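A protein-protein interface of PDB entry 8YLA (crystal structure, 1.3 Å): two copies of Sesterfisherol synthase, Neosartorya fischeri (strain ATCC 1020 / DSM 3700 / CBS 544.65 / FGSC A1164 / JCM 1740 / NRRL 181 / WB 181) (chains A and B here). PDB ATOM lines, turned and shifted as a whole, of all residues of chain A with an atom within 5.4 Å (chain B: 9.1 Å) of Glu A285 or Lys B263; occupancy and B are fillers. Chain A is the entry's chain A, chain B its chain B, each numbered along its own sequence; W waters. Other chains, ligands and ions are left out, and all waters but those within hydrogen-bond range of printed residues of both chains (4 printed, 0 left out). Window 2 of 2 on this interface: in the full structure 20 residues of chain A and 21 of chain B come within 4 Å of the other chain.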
ATOM      1  N   GLN A 281       7.983 -13.152 -13.074  1.00  0.00           N
ATOM      2  CA  GLN A 281       9.106 -13.488 -13.944  1.00  0.00           C
ATOM      3  C   GLN A 281       8.735 -13.328 -15.411  1.00  0.00           C
ATOM      4  O   GLN A 281       9.549 -12.868 -16.219  1.00  0.00           O
ATOM      5  CB  GLN A 281       9.596 -14.912 -13.669  1.00  0.00           C
ATOM      6  CG  GLN A 281      10.613 -15.439 -14.690  1.00  0.00           C
ATOM      7  CD  GLN A 281      11.918 -14.673 -14.644  1.00  0.00           C
ATOM      8  OE1 GLN A 281      12.474 -14.436 -13.570  1.00  0.00           O
ATOM      9  NE2 GLN A 281      12.416 -14.273 -15.816  1.00  0.00           N
ATOM     10  N   GLN A 282       7.513 -13.711 -15.778  1.00  0.00           N
ATOM     11  CA  GLN A 282       7.081 -13.528 -17.156  1.00  0.00           C
ATOM     12  C   GLN A 282       7.077 -12.052 -17.545  1.00  0.00           C
ATOM     13  O   GLN A 282       7.522 -11.691 -18.644  1.00  0.00           O
ATOM     14  CB  GLN A 282       5.704 -14.147 -17.357  1.00  0.00           C
ATOM     15  CG  GLN A 282       5.215 -14.129 -18.785  1.00  0.00           C
ATOM     16  CD  GLN A 282       4.085 -15.109 -18.982  1.00  0.00           C
ATOM     17  OE1 GLN A 282       3.116 -15.101 -18.227  1.00  0.00           O
ATOM     18  NE2 GLN A 282       4.234 -16.006 -19.951  1.00  0.00           N
ATOM     19  N   TYR A 283       6.580 -11.175 -16.656  1.00  0.00           N
ATOM     20  CA  TYR A 283       6.678  -9.738 -16.886  1.00  0.00           C
ATOM     21  C   TYR A 283       8.110  -9.315 -17.208  1.00  0.00           C
ATOM     22  O   TYR A 283       8.343  -8.557 -18.153  1.00  0.00           O
ATOM     23  CB  TYR A 283       6.126  -8.979 -15.675  1.00  0.00           C
ATOM     24  CG  TYR A 283       6.656  -7.568 -15.532  1.00  0.00           C
ATOM     25  CD1 TYR A 283       6.240  -6.547 -16.385  1.00  0.00           C
ATOM     26  CD2 TYR A 283       7.535  -7.243 -14.513  1.00  0.00           C
ATOM     27  CE1 TYR A 283       6.731  -5.238 -16.242  1.00  0.00           C
ATOM     28  CE2 TYR A 283       8.028  -5.965 -14.360  1.00  0.00           C
ATOM     29  CZ  TYR A 283       7.613  -4.967 -15.216  1.00  0.00           C
ATOM     30  OH  TYR A 283       8.104  -3.694 -15.038  1.00  0.00           O
ATOM     31  N   LEU A 284       9.083  -9.798 -16.436  1.00  0.00           N
ATOM     32  CA  LEU A 284      10.476  -9.432 -16.721  1.00  0.00           C
ATOM     33  C   LEU A 284      10.895  -9.873 -18.121  1.00  0.00           C
ATOM     34  O   LEU A 284      11.562  -9.120 -18.847  1.00  0.00           O
ATOM     35  CB  LEU A 284      11.425 -10.005 -15.662  1.00  0.00           C
ATOM     36  CG  LEU A 284      11.213  -9.512 -14.229  1.00  0.00           C
ATOM     37  CD1 LEU A 284      12.145 -10.240 -13.266  1.00  0.00           C
ATOM     38  CD2 LEU A 284      11.385  -7.996 -14.128  1.00  0.00           C
ATOM     39  N   GLU A 285      10.504 -11.080 -18.524  1.00  0.00           N
ATOM     40  CA  GLU A 285      10.881 -11.581 -19.841  1.00  0.00           C
ATOM     41  C   GLU A 285      10.198 -10.794 -20.949  1.00  0.00           C
ATOM     42  O   GLU A 285      10.814 -10.493 -21.981  1.00  0.00           O
ATOM     43  CB  GLU A 285      10.535 -13.060 -19.931  1.00  0.00           C
ATOM     44  CG  GLU A 285      11.395 -13.886 -19.016  1.00  0.00           C
ATOM     45  CD  GLU A 285      11.107 -15.369 -19.107  1.00  0.00           C
ATOM     46  OE1 GLU A 285      10.134 -15.750 -19.794  1.00  0.00           O
ATOM     47  OE2 GLU A 285      11.841 -16.153 -18.468  1.00  0.00           O
ATOM     48  N   ARG A 286       8.928 -10.435 -20.750  1.00  0.00           N
ATOM     49  CA  ARG A 286       8.217  -9.649 -21.749  1.00  0.00           C
ATOM     50  C   ARG A 286       8.807  -8.251 -21.854  1.00  0.00           C
ATOM     51  O   ARG A 286       8.894  -7.682 -22.950  1.00  0.00           O
ATOM     52  CB  ARG A 286       6.736  -9.571 -21.372  1.00  0.00           C
ATOM     53  CG  ARG A 286       6.005 -10.922 -21.254  1.00  0.00           C
ATOM     54  CD  ARG A 286       5.643 -11.528 -22.614  1.00  0.00           C
ATOM     55  NE  ARG A 286       4.977 -12.826 -22.490  1.00  0.00           N
ATOM     56  CZ  ARG A 286       3.662 -12.986 -22.414  1.00  0.00           C
ATOM     57  NH1 ARG A 286       2.838 -11.954 -22.378  1.00  0.00           N
ATOM     58  NH2 ARG A 286       3.161 -14.218 -22.396  1.00  0.00           N
ATOM     59  N   LYS A 287       9.190  -7.672 -20.719  1.00  0.00           N
ATOM     60  CA  LYS A 287       9.757  -6.325 -20.714  1.00  0.00           C
ATOM     61  C   LYS A 287      11.119  -6.305 -21.405  1.00  0.00           C
ATOM     62  O   LYS A 287      11.384  -5.432 -22.240  1.00  0.00           O
ATOM     63  CB  LYS A 287       9.844  -5.829 -19.269  1.00  0.00           C
ATOM     64  CG  LYS A 287      10.727  -4.628 -19.016  1.00  0.00           C
ATOM     65  CD  LYS A 287      10.519  -4.081 -17.596  1.00  0.00           C
ATOM     66  CE  LYS A 287      11.203  -4.914 -16.523  1.00  0.00           C
ATOM     67  NZ  LYS A 287      11.211  -4.214 -15.195  1.00  0.00           N
ATOM     68  N   ARG A 288      11.980  -7.275 -21.081  1.00  0.00           N
ATOM     69  CA  ARG A 288      13.266  -7.389 -21.773  1.00  0.00           C
ATOM     70  C   ARG A 288      13.088  -7.480 -23.282  1.00  0.00           C
ATOM     71  O   ARG A 288      13.843  -6.857 -24.039  1.00  0.00           O
ATOM     72  CB  ARG A 288      14.069  -8.585 -21.243  1.00  0.00           C
ATOM     73  CG  ARG A 288      14.603  -8.388 -19.835  1.00  0.00           C
ATOM     74  CD  ARG A 288      15.640  -9.430 -19.425  1.00  0.00           C
ATOM     75  NE  ARG A 288      15.062 -10.750 -19.200  1.00  0.00           N
ATOM     76  CZ  ARG A 288      14.935 -11.312 -18.005  1.00  0.00           C
ATOM     77  NH1 ARG A 288      15.351 -10.700 -16.908  1.00  0.00           N
ATOM     78  NH2 ARG A 288      14.364 -12.509 -17.909  1.00  0.00           N
ATOM     79  N   ALA A 289      12.096  -8.245 -23.744  1.00  0.00           N
ATOM     80  CA  ALA A 289      11.854  -8.368 -25.178  1.00  0.00           C
ATOM     81  C   ALA A 289      11.481  -7.031 -25.806  1.00  0.00           C
ATOM     82  O   ALA A 289      11.955  -6.695 -26.901  1.00  0.00           O
ATOM     83  CB  ALA A 289      10.777  -9.421 -25.445  1.00  0.00           C
ATOM     84  N   ILE A 290      10.617  -6.255 -25.147  1.00  0.00           N
ATOM     85  CA  ILE A 290      10.265  -4.945 -25.680  1.00  0.00           C
ATOM     86  C   ILE A 290      11.503  -4.075 -25.842  1.00  0.00           C
ATOM     87  O   ILE A 290      11.684  -3.426 -26.879  1.00  0.00           O
ATOM     88  CB  ILE A 290       9.183  -4.251 -24.831  1.00  0.00           C
ATOM     89  CG1 ILE A 290       7.827  -4.941 -25.015  1.00  0.00           C
ATOM     90  CG2 ILE A 290       9.094  -2.770 -25.201  1.00  0.00           C
ATOM     91  CD1 ILE A 290       6.761  -4.503 -24.016  1.00  0.00           C
ATOM     92  N   PHE B 236       5.128 -26.634 -35.567  1.00  0.00           N
ATOM     93  CA  PHE B 236       5.861 -25.378 -35.729  1.00  0.00           C
ATOM     94  C   PHE B 236       6.915 -25.464 -36.831  1.00  0.00           C
ATOM     95  O   PHE B 236       7.008 -24.563 -37.673  1.00  0.00           O
ATOM     96  CB  PHE B 236       6.519 -24.933 -34.422  1.00  0.00           C
ATOM     97  CG  PHE B 236       7.416 -23.749 -34.620  1.00  0.00           C
ATOM     98  CD1 PHE B 236       6.893 -22.468 -34.690  1.00  0.00           C
ATOM     99  CD2 PHE B 236       8.772 -23.930 -34.856  1.00  0.00           C
ATOM    100  CE1 PHE B 236       7.711 -21.379 -34.930  1.00  0.00           C
ATOM    101  CE2 PHE B 236       9.598 -22.847 -35.111  1.00  0.00           C
ATOM    102  CZ  PHE B 236       9.065 -21.567 -35.155  1.00  0.00           C
ATOM    103  N   VAL B 253       1.501 -20.930 -31.304  1.00  0.00           N
ATOM    104  CA  VAL B 253       1.876 -20.359 -30.010  1.00  0.00           C
ATOM    105  C   VAL B 253       3.387 -20.328 -29.817  1.00  0.00           C
ATOM    106  O   VAL B 253       3.910 -19.435 -29.132  1.00  0.00           O
ATOM    107  CB  VAL B 253       1.155 -21.066 -28.842  1.00  0.00           C
ATOM    108  CG1 VAL B 253       1.788 -22.406 -28.513  1.00  0.00           C
ATOM    109  CG2 VAL B 253       1.147 -20.168 -27.602  1.00  0.00           C
ATOM    110  N   VAL B 254       4.120 -21.271 -30.421  1.00  0.00           N
ATOM    111  CA  VAL B 254       5.580 -21.231 -30.343  1.00  0.00           C
ATOM    112  C   VAL B 254       6.098 -19.951 -30.968  1.00  0.00           C
ATOM    113  O   VAL B 254       7.010 -19.305 -30.440  1.00  0.00           O
ATOM    114  CB  VAL B 254       6.212 -22.469 -31.008  1.00  0.00           C
ATOM    115  CG1 VAL B 254       7.732 -22.338 -31.030  1.00  0.00           C
ATOM    116  CG2 VAL B 254       5.813 -23.732 -30.302  1.00  0.00           C
ATOM    117  N   GLU B 255       5.522 -19.567 -32.110  1.00  0.00           N
ATOM    118  CA  GLU B 255       5.920 -18.328 -32.759  1.00  0.00           C
ATOM    119  C   GLU B 255       5.589 -17.121 -31.898  1.00  0.00           C
ATOM    120  O   GLU B 255       6.376 -16.169 -31.820  1.00  0.00           O
ATOM    121  CB  GLU B 255       5.260 -18.212 -34.130  1.00  0.00           C
ATOM    122  CG  GLU B 255       5.628 -16.928 -34.859  1.00  0.00           C
ATOM    123  CD  GLU B 255       7.085 -16.861 -35.286  1.00  0.00           C
ATOM    124  OE1 GLU B 255       7.819 -17.863 -35.164  1.00  0.00           O
ATOM    125  OE2 GLU B 255       7.494 -15.762 -35.731  1.00  0.00           O
ATOM    126  N   VAL B 256       4.419 -17.132 -31.256  1.00  0.00           N
ATOM    127  CA  VAL B 256       4.055 -16.014 -30.391  1.00  0.00           C
ATOM    128  C   VAL B 256       5.065 -15.869 -29.263  1.00  0.00           C
ATOM    129  O   VAL B 256       5.554 -14.768 -28.981  1.00  0.00           O
ATOM    130  CB  VAL B 256       2.619 -16.176 -29.867  1.00  0.00           C
ATOM    131  CG1 VAL B 256       2.276 -15.032 -28.908  1.00  0.00           C
ATOM    132  CG2 VAL B 256       1.644 -16.235 -31.029  1.00  0.00           C
ATOM    133  N   VAL B 257       5.398 -16.977 -28.613  1.00  0.00           N
ATOM    134  CA  VAL B 257       6.370 -16.950 -27.521  1.00  0.00           C
ATOM    135  C   VAL B 257       7.737 -16.471 -28.013  1.00  0.00           C
ATOM    136  O   VAL B 257       8.395 -15.659 -27.349  1.00  0.00           O
ATOM    137  CB  VAL B 257       6.449 -18.341 -26.858  1.00  0.00           C
ATOM    138  CG1 VAL B 257       7.634 -18.399 -25.894  1.00  0.00           C
ATOM    139  CG2 VAL B 257       5.140 -18.673 -26.137  1.00  0.00           C
ATOM    140  N   ARG B 258       8.190 -16.965 -29.177  1.00  0.00           N
ATOM    141  CA  ARG B 258       9.445 -16.493 -29.766  1.00  0.00           C
ATOM    142  C   ARG B 258       9.477 -14.976 -29.821  1.00  0.00           C
ATOM    143  O   ARG B 258      10.467 -14.338 -29.435  1.00  0.00           O
ATOM    144  CB  ARG B 258       9.581 -16.996 -31.208  1.00  0.00           C
ATOM    145  CG  ARG B 258      10.110 -18.383 -31.435  1.00  0.00           C
ATOM    146  CD  ARG B 258      10.193 -18.645 -32.953  1.00  0.00           C
ATOM    147  NE  ARG B 258      11.336 -18.017 -33.617  1.00  0.00           N
ATOM    148  CZ  ARG B 258      11.472 -17.901 -34.934  1.00  0.00           C
ATOM    149  NH1 ARG B 258      10.489 -18.208 -35.766  1.00  0.00           N
ATOM    150  NH2 ARG B 258      12.631 -17.477 -35.436  1.00  0.00           N
ATOM    151  N   GLN B 259       8.405 -14.386 -30.341  1.00  0.00           N
ATOM    152  CA  GLN B 259       8.350 -12.948 -30.550  1.00  0.00           C
ATOM    153  C   GLN B 259       8.227 -12.193 -29.231  1.00  0.00           C
ATOM    154  O   GLN B 259       9.066 -11.347 -28.903  1.00  0.00           O
ATOM    155  CB  GLN B 259       7.191 -12.620 -31.497  1.00  0.00           C
ATOM    156  CG  GLN B 259       7.390 -13.084 -32.948  1.00  0.00           C
ATOM    157  CD  GLN B 259       6.239 -12.676 -33.851  1.00  0.00           C
ATOM    158  OE1 GLN B 259       5.554 -11.687 -33.588  1.00  0.00           O
ATOM    159  NE2 GLN B 259       6.059 -13.402 -34.957  1.00  0.00           N
ATOM    160  N   ILE B 260       7.198 -12.496 -28.437  1.00  0.00           N
ATOM    161  CA  ILE B 260       6.905 -11.648 -27.282  1.00  0.00           C
ATOM    162  C   ILE B 260       7.833 -11.899 -26.112  1.00  0.00           C
ATOM    163  O   ILE B 260       7.833 -11.110 -25.162  1.00  0.00           O
ATOM    164  CB  ILE B 260       5.414 -11.631 -26.896  1.00  0.00           C
ATOM    165  CG1 ILE B 260       4.983 -12.942 -26.236  1.00  0.00           C
ATOM    166  CG2 ILE B 260       4.571 -11.297 -28.120  1.00  0.00           C
ATOM    167  CD1 ILE B 260       3.510 -12.934 -25.828  1.00  0.00           C
ATOM    168  N   GLU B 261       8.638 -12.957 -26.154  1.00  0.00           N
ATOM    169  CA  GLU B 261       9.626 -13.182 -25.113  1.00  0.00           C
ATOM    170  C   GLU B 261      11.053 -13.143 -25.636  1.00  0.00           C
ATOM    171  O   GLU B 261      11.982 -13.422 -24.872  1.00  0.00           O
ATOM    172  CB  GLU B 261       9.312 -14.455 -24.317  1.00  0.00           C
ATOM    173  CG  GLU B 261       8.049 -14.231 -23.485  1.00  0.00           C
ATOM    174  CD  GLU B 261       7.573 -15.421 -22.681  1.00  0.00           C
ATOM    175  OE1 GLU B 261       8.261 -16.463 -22.635  1.00  0.00           O
ATOM    176  OE2 GLU B 261       6.487 -15.288 -22.075  1.00  0.00           O
ATOM    177  N   ASN B 262      11.254 -12.756 -26.896  1.00  0.00           N
ATOM    178  CA  ASN B 262      12.595 -12.659 -27.470  1.00  0.00           C
ATOM    179  C   ASN B 262      13.381 -13.947 -27.218  1.00  0.00           C
ATOM    180  O   ASN B 262      14.508 -13.930 -26.711  1.00  0.00           O
ATOM    181  CB  ASN B 262      13.328 -11.430 -26.917  1.00  0.00           C
ATOM    182  CG  ASN B 262      14.673 -11.181 -27.580  1.00  0.00           C
ATOM    183  OD1 ASN B 262      14.842 -11.395 -28.780  1.00  0.00           O
ATOM    184  ND2 ASN B 262      15.652 -10.767 -26.777  1.00  0.00           N
ATOM    185  N   LYS B 263      12.758 -15.078 -27.549  1.00  0.00           N
ATOM    186  CA  LYS B 263      13.318 -16.401 -27.311  1.00  0.00           C
ATOM    187  C   LYS B 263      13.700 -17.034 -28.639  1.00  0.00           C
ATOM    188  O   LYS B 263      13.046 -16.810 -29.661  1.00  0.00           O
ATOM    189  CB  LYS B 263      12.303 -17.321 -26.625  1.00  0.00           C
ATOM    190  CG  LYS B 263      12.227 -17.175 -25.123  1.00  0.00           C
ATOM    191  CD  LYS B 263      11.161 -18.097 -24.552  1.00  0.00           C
ATOM    192  CE  LYS B 263      11.314 -18.326 -23.058  1.00  0.00           C
ATOM    193  NZ  LYS B 263      10.997 -17.112 -22.263  1.00  0.00           N
ATOM    194  N   SER B 264      14.768 -17.825 -28.622  1.00  0.00           N
ATOM    195  CA  SER B 264      15.096 -18.658 -29.769  1.00  0.00           C
ATOM    196  C   SER B 264      14.014 -19.726 -29.971  1.00  0.00           C
ATOM    197  O   SER B 264      13.156 -19.965 -29.109  1.00  0.00           O
ATOM    198  CB  SER B 264      16.434 -19.350 -29.530  1.00  0.00           C
ATOM    199  OG  SER B 264      16.261 -20.365 -28.554  1.00  0.00           O
ATOM    200  N   ILE B 265      14.061 -20.385 -31.131  1.00  0.00           N
ATOM    201  CA  ILE B 265      13.117 -21.472 -31.393  1.00  0.00           C
ATOM    202  C   ILE B 265      13.182 -22.520 -30.287  1.00  0.00           C
ATOM    203  O   ILE B 265      12.152 -22.961 -29.767  1.00  0.00           O
ATOM    204  CB  ILE B 265      13.358 -22.084 -32.782  1.00  0.00           C
ATOM    205  CG1 ILE B 265      12.991 -21.076 -33.868  1.00  0.00           C
ATOM    206  CG2 ILE B 265      12.567 -23.380 -32.937  1.00  0.00           C
ATOM    207  CD1 ILE B 265      13.407 -21.488 -35.255  1.00  0.00           C
ATOM    208  N   ASP B 266      14.396 -22.929 -29.895  1.00  0.00           N
ATOM    209  CA  ASP B 266      14.496 -23.987 -28.899  1.00  0.00           C
ATOM    210  C   ASP B 266      14.044 -23.521 -27.520  1.00  0.00           C
ATOM    211  O   ASP B 266      13.432 -24.297 -26.775  1.00  0.00           O
ATOM    212  CB  ASP B 266      15.902 -24.580 -28.885  1.00  0.00           C
ATOM    213  CG  ASP B 266      16.189 -25.365 -30.140  1.00  0.00           C
ATOM    214  OD1 ASP B 266      15.291 -26.114 -30.586  1.00  0.00           O
ATOM    215  OD2 ASP B 266      17.280 -25.199 -30.715  1.00  0.00           O
ATOM    216  N   GLU B 267      14.297 -22.249 -27.177  1.00  0.00           N
ATOM    217  CA  GLU B 267      13.808 -21.720 -25.907  1.00  0.00           C
ATOM    218  C   GLU B 267      12.287 -21.641 -25.898  1.00  0.00           C
ATOM    219  O   GLU B 267      11.647 -21.928 -24.879  1.00  0.00           O
ATOM    220  CB  GLU B 267      14.424 -20.340 -25.631  1.00  0.00           C
ATOM    221  CG  GLU B 267      15.937 -20.377 -25.424  1.00  0.00           C
ATOM    222  CD  GLU B 267      16.621 -19.021 -25.548  1.00  0.00           C
ATOM    223  OE1 GLU B 267      16.000 -18.043 -26.019  1.00  0.00           O
ATOM    224  OE2 GLU B 267      17.815 -18.945 -25.199  1.00  0.00           O
ATOM    225  N   ALA B 268      11.693 -21.213 -27.017  1.00  0.00           N
ATOM    226  CA  ALA B 268      10.239 -21.142 -27.105  1.00  0.00           C
ATOM    227  C   ALA B 268       9.622 -22.530 -27.054  1.00  0.00           C
ATOM    228  O   ALA B 268       8.619 -22.743 -26.366  1.00  0.00           O
ATOM    229  CB  ALA B 268       9.825 -20.392 -28.371  1.00  0.00           C
ATOM    230  N   LYS B 269      10.223 -23.499 -27.749  1.00  0.00           N
ATOM    231  CA  LYS B 269       9.727 -24.868 -27.671  1.00  0.00           C
ATOM    232  C   LYS B 269       9.800 -25.406 -26.248  1.00  0.00           C
ATOM    233  O   LYS B 269       8.861 -26.055 -25.775  1.00  0.00           O
ATOM    234  CB  LYS B 269      10.526 -25.769 -28.606  1.00  0.00           C
ATOM    235  CG  LYS B 269      10.201 -25.589 -30.068  1.00  0.00           C
ATOM    236  CD  LYS B 269      11.023 -26.576 -30.867  1.00  0.00           C
ATOM    237  CE  LYS B 269      10.658 -26.577 -32.342  1.00  0.00           C
ATOM    238  NZ  LYS B 269      11.569 -27.495 -33.112  1.00  0.00           N
ATOM    239  N   ALA B 270      10.903 -25.147 -25.546  1.00  0.00           N
ATOM    240  CA  ALA B 270      11.030 -25.648 -24.184  1.00  0.00           C
ATOM    241  C   ALA B 270       9.947 -25.064 -23.292  1.00  0.00           C
ATOM    242  O   ALA B 270       9.381 -25.766 -22.442  1.00  0.00           O
ATOM    243  CB  ALA B 270      12.419 -25.331 -23.634  1.00  0.00           C
ATOM    244  N   ALA B 271       9.634 -23.779 -23.486  1.00  0.00           N
ATOM    245  CA  ALA B 271       8.579 -23.153 -22.699  1.00  0.00           C
ATOM    246  C   ALA B 271       7.221 -23.770 -23.007  1.00  0.00           C
ATOM    247  O   ALA B 271       6.420 -24.003 -22.097  1.00  0.00           O
ATOM    248  CB  ALA B 271       8.560 -21.641 -22.935  1.00  0.00           C
ATOM    249  N   VAL B 272       6.938 -24.028 -24.287  1.00  0.00           N
ATOM    250  CA  VAL B 272       5.649 -24.601 -24.656  1.00  0.00           C
ATOM    251  C   VAL B 272       5.515 -26.029 -24.142  1.00  0.00           C
ATOM    252  O   VAL B 272       4.433 -26.429 -23.690  1.00  0.00           O
ATOM    253  CB  VAL B 272       5.395 -24.451 -26.165  1.00  0.00           C
ATOM    254  CG1 VAL B 272       4.122 -25.159 -26.573  1.00  0.00           C
ATOM    255  CG2 VAL B 272       5.287 -22.959 -26.507  1.00  0.00           C
HETATM  256  O   HOH W   1      13.095 -11.730 -22.910  1.00  0.00           O
HETATM  257  O   HOH W   2       4.419 -16.595 -23.238  1.00  0.00           O
HETATM  258  O   HOH W   3      14.957 -10.095 -24.379  1.00  0.00           O
HETATM  259  O   HOH W   4       7.296  -8.468 -25.135  1.00  0.00           O
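OE2 of Glu B261 sits at hydrogen-bond distance from NE2 of Gln A282 (3.2 Å).
The side-chain carboxylate (OE1) of Glu B261 sits close to the side-chain carboxylate (OE1) of Glu A285 (3.5 Å).
The side-chain carboxylate (OE1) of Glu A285 lies within salt-bridge range of the side-chain amino group (NZ) of Lys B263, 2.9 Å away.
The side-chain carboxylate (OE2) of Glu B261 lies within salt-bridge range of the guanidinium group (NE) of Arg A286 (2.9 Å).
The side-chain amide nitrogen (NE2) of Gln A281 sits at hydrogen-bond distance from the side-chain carboxylate (OE2) of Glu A285, at 3.3 Å.
The side-chain amino group (NZ) of Lys B263 lies within salt-bridge range of the side-chain carboxylate (OE1) of Glu B261, at 2.8 Å.
NE2 of Gln A282 sits close to NH2 of Arg A286.
O of Arg B258 lies within hydrogen-bond range of N of Lys B263, 3.1 Å away.
Among the printed residues, merely in contact across the chains: Arg A286 with Ile B260, Ala A289 with Ile B260, Ala A289 with Asn B262 and Ala A289 with Glu B261.
Printed residues of chain B within 4 Å of Gln A282: Glu B261 (3.2 Å).
Glu A285 touches just these residues of chain B: Glu B261 (3.5 Å) and Lys B263 (2.9 Å).
Of the printed residues of chain A, Glu B261 touches Gln A282 (3.2 Å), Glu A285 (3.5 Å), Arg A286 (2.9 Å) and Ala A289 (3.7 Å).
Lys B263 touches one residue of chain A.
Val B272 touches none of the printed residues of chain A.
The nearest residue of chain B that does not touch Glu A285 is Ile B260 (4.4 Å).
Of the 10 printed residues of chain A, 4 touch a printed residue of chain B.
Of the 21 printed residues of chain B, 4 touch a printed residue of chain A.
Hydrophobic or aromatic side chains of chain B that line the printed part of chain A: Ile B260.
Among the printed residues, 8 pairs touch across the chains.
No position is printed for both chains.
Of the 8 pairs that touch across the chains among the printed residues, none has its exchanged pair printed and touching as well.
Water W3 lies within hydrogen-bond range of ND2 of Asn B262 (2.6 Å), O of Arg A288 (3.4 Å) and N of Ala A289 (3.5 Å).
Water W4 lies within hydrogen-bond range of the backbone carbonyl oxygen (O) of Ile B260 (2.7 Å) and the backbone carbonyl oxygen (O) of Arg A286 (2.8 Å).
Water W2 lies within hydrogen-bond range of OE2 of Glu B261 (2.7 Å), NH2 of Arg A286 (2.8 Å) and NE2 of Gln A282 (3.3 Å).
Water W1 bridges the backbone carbonyl oxygen of Glu A285 (2.8 Å) and the backbone carbonyl oxygen of Glu B261 (2.8 Å).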
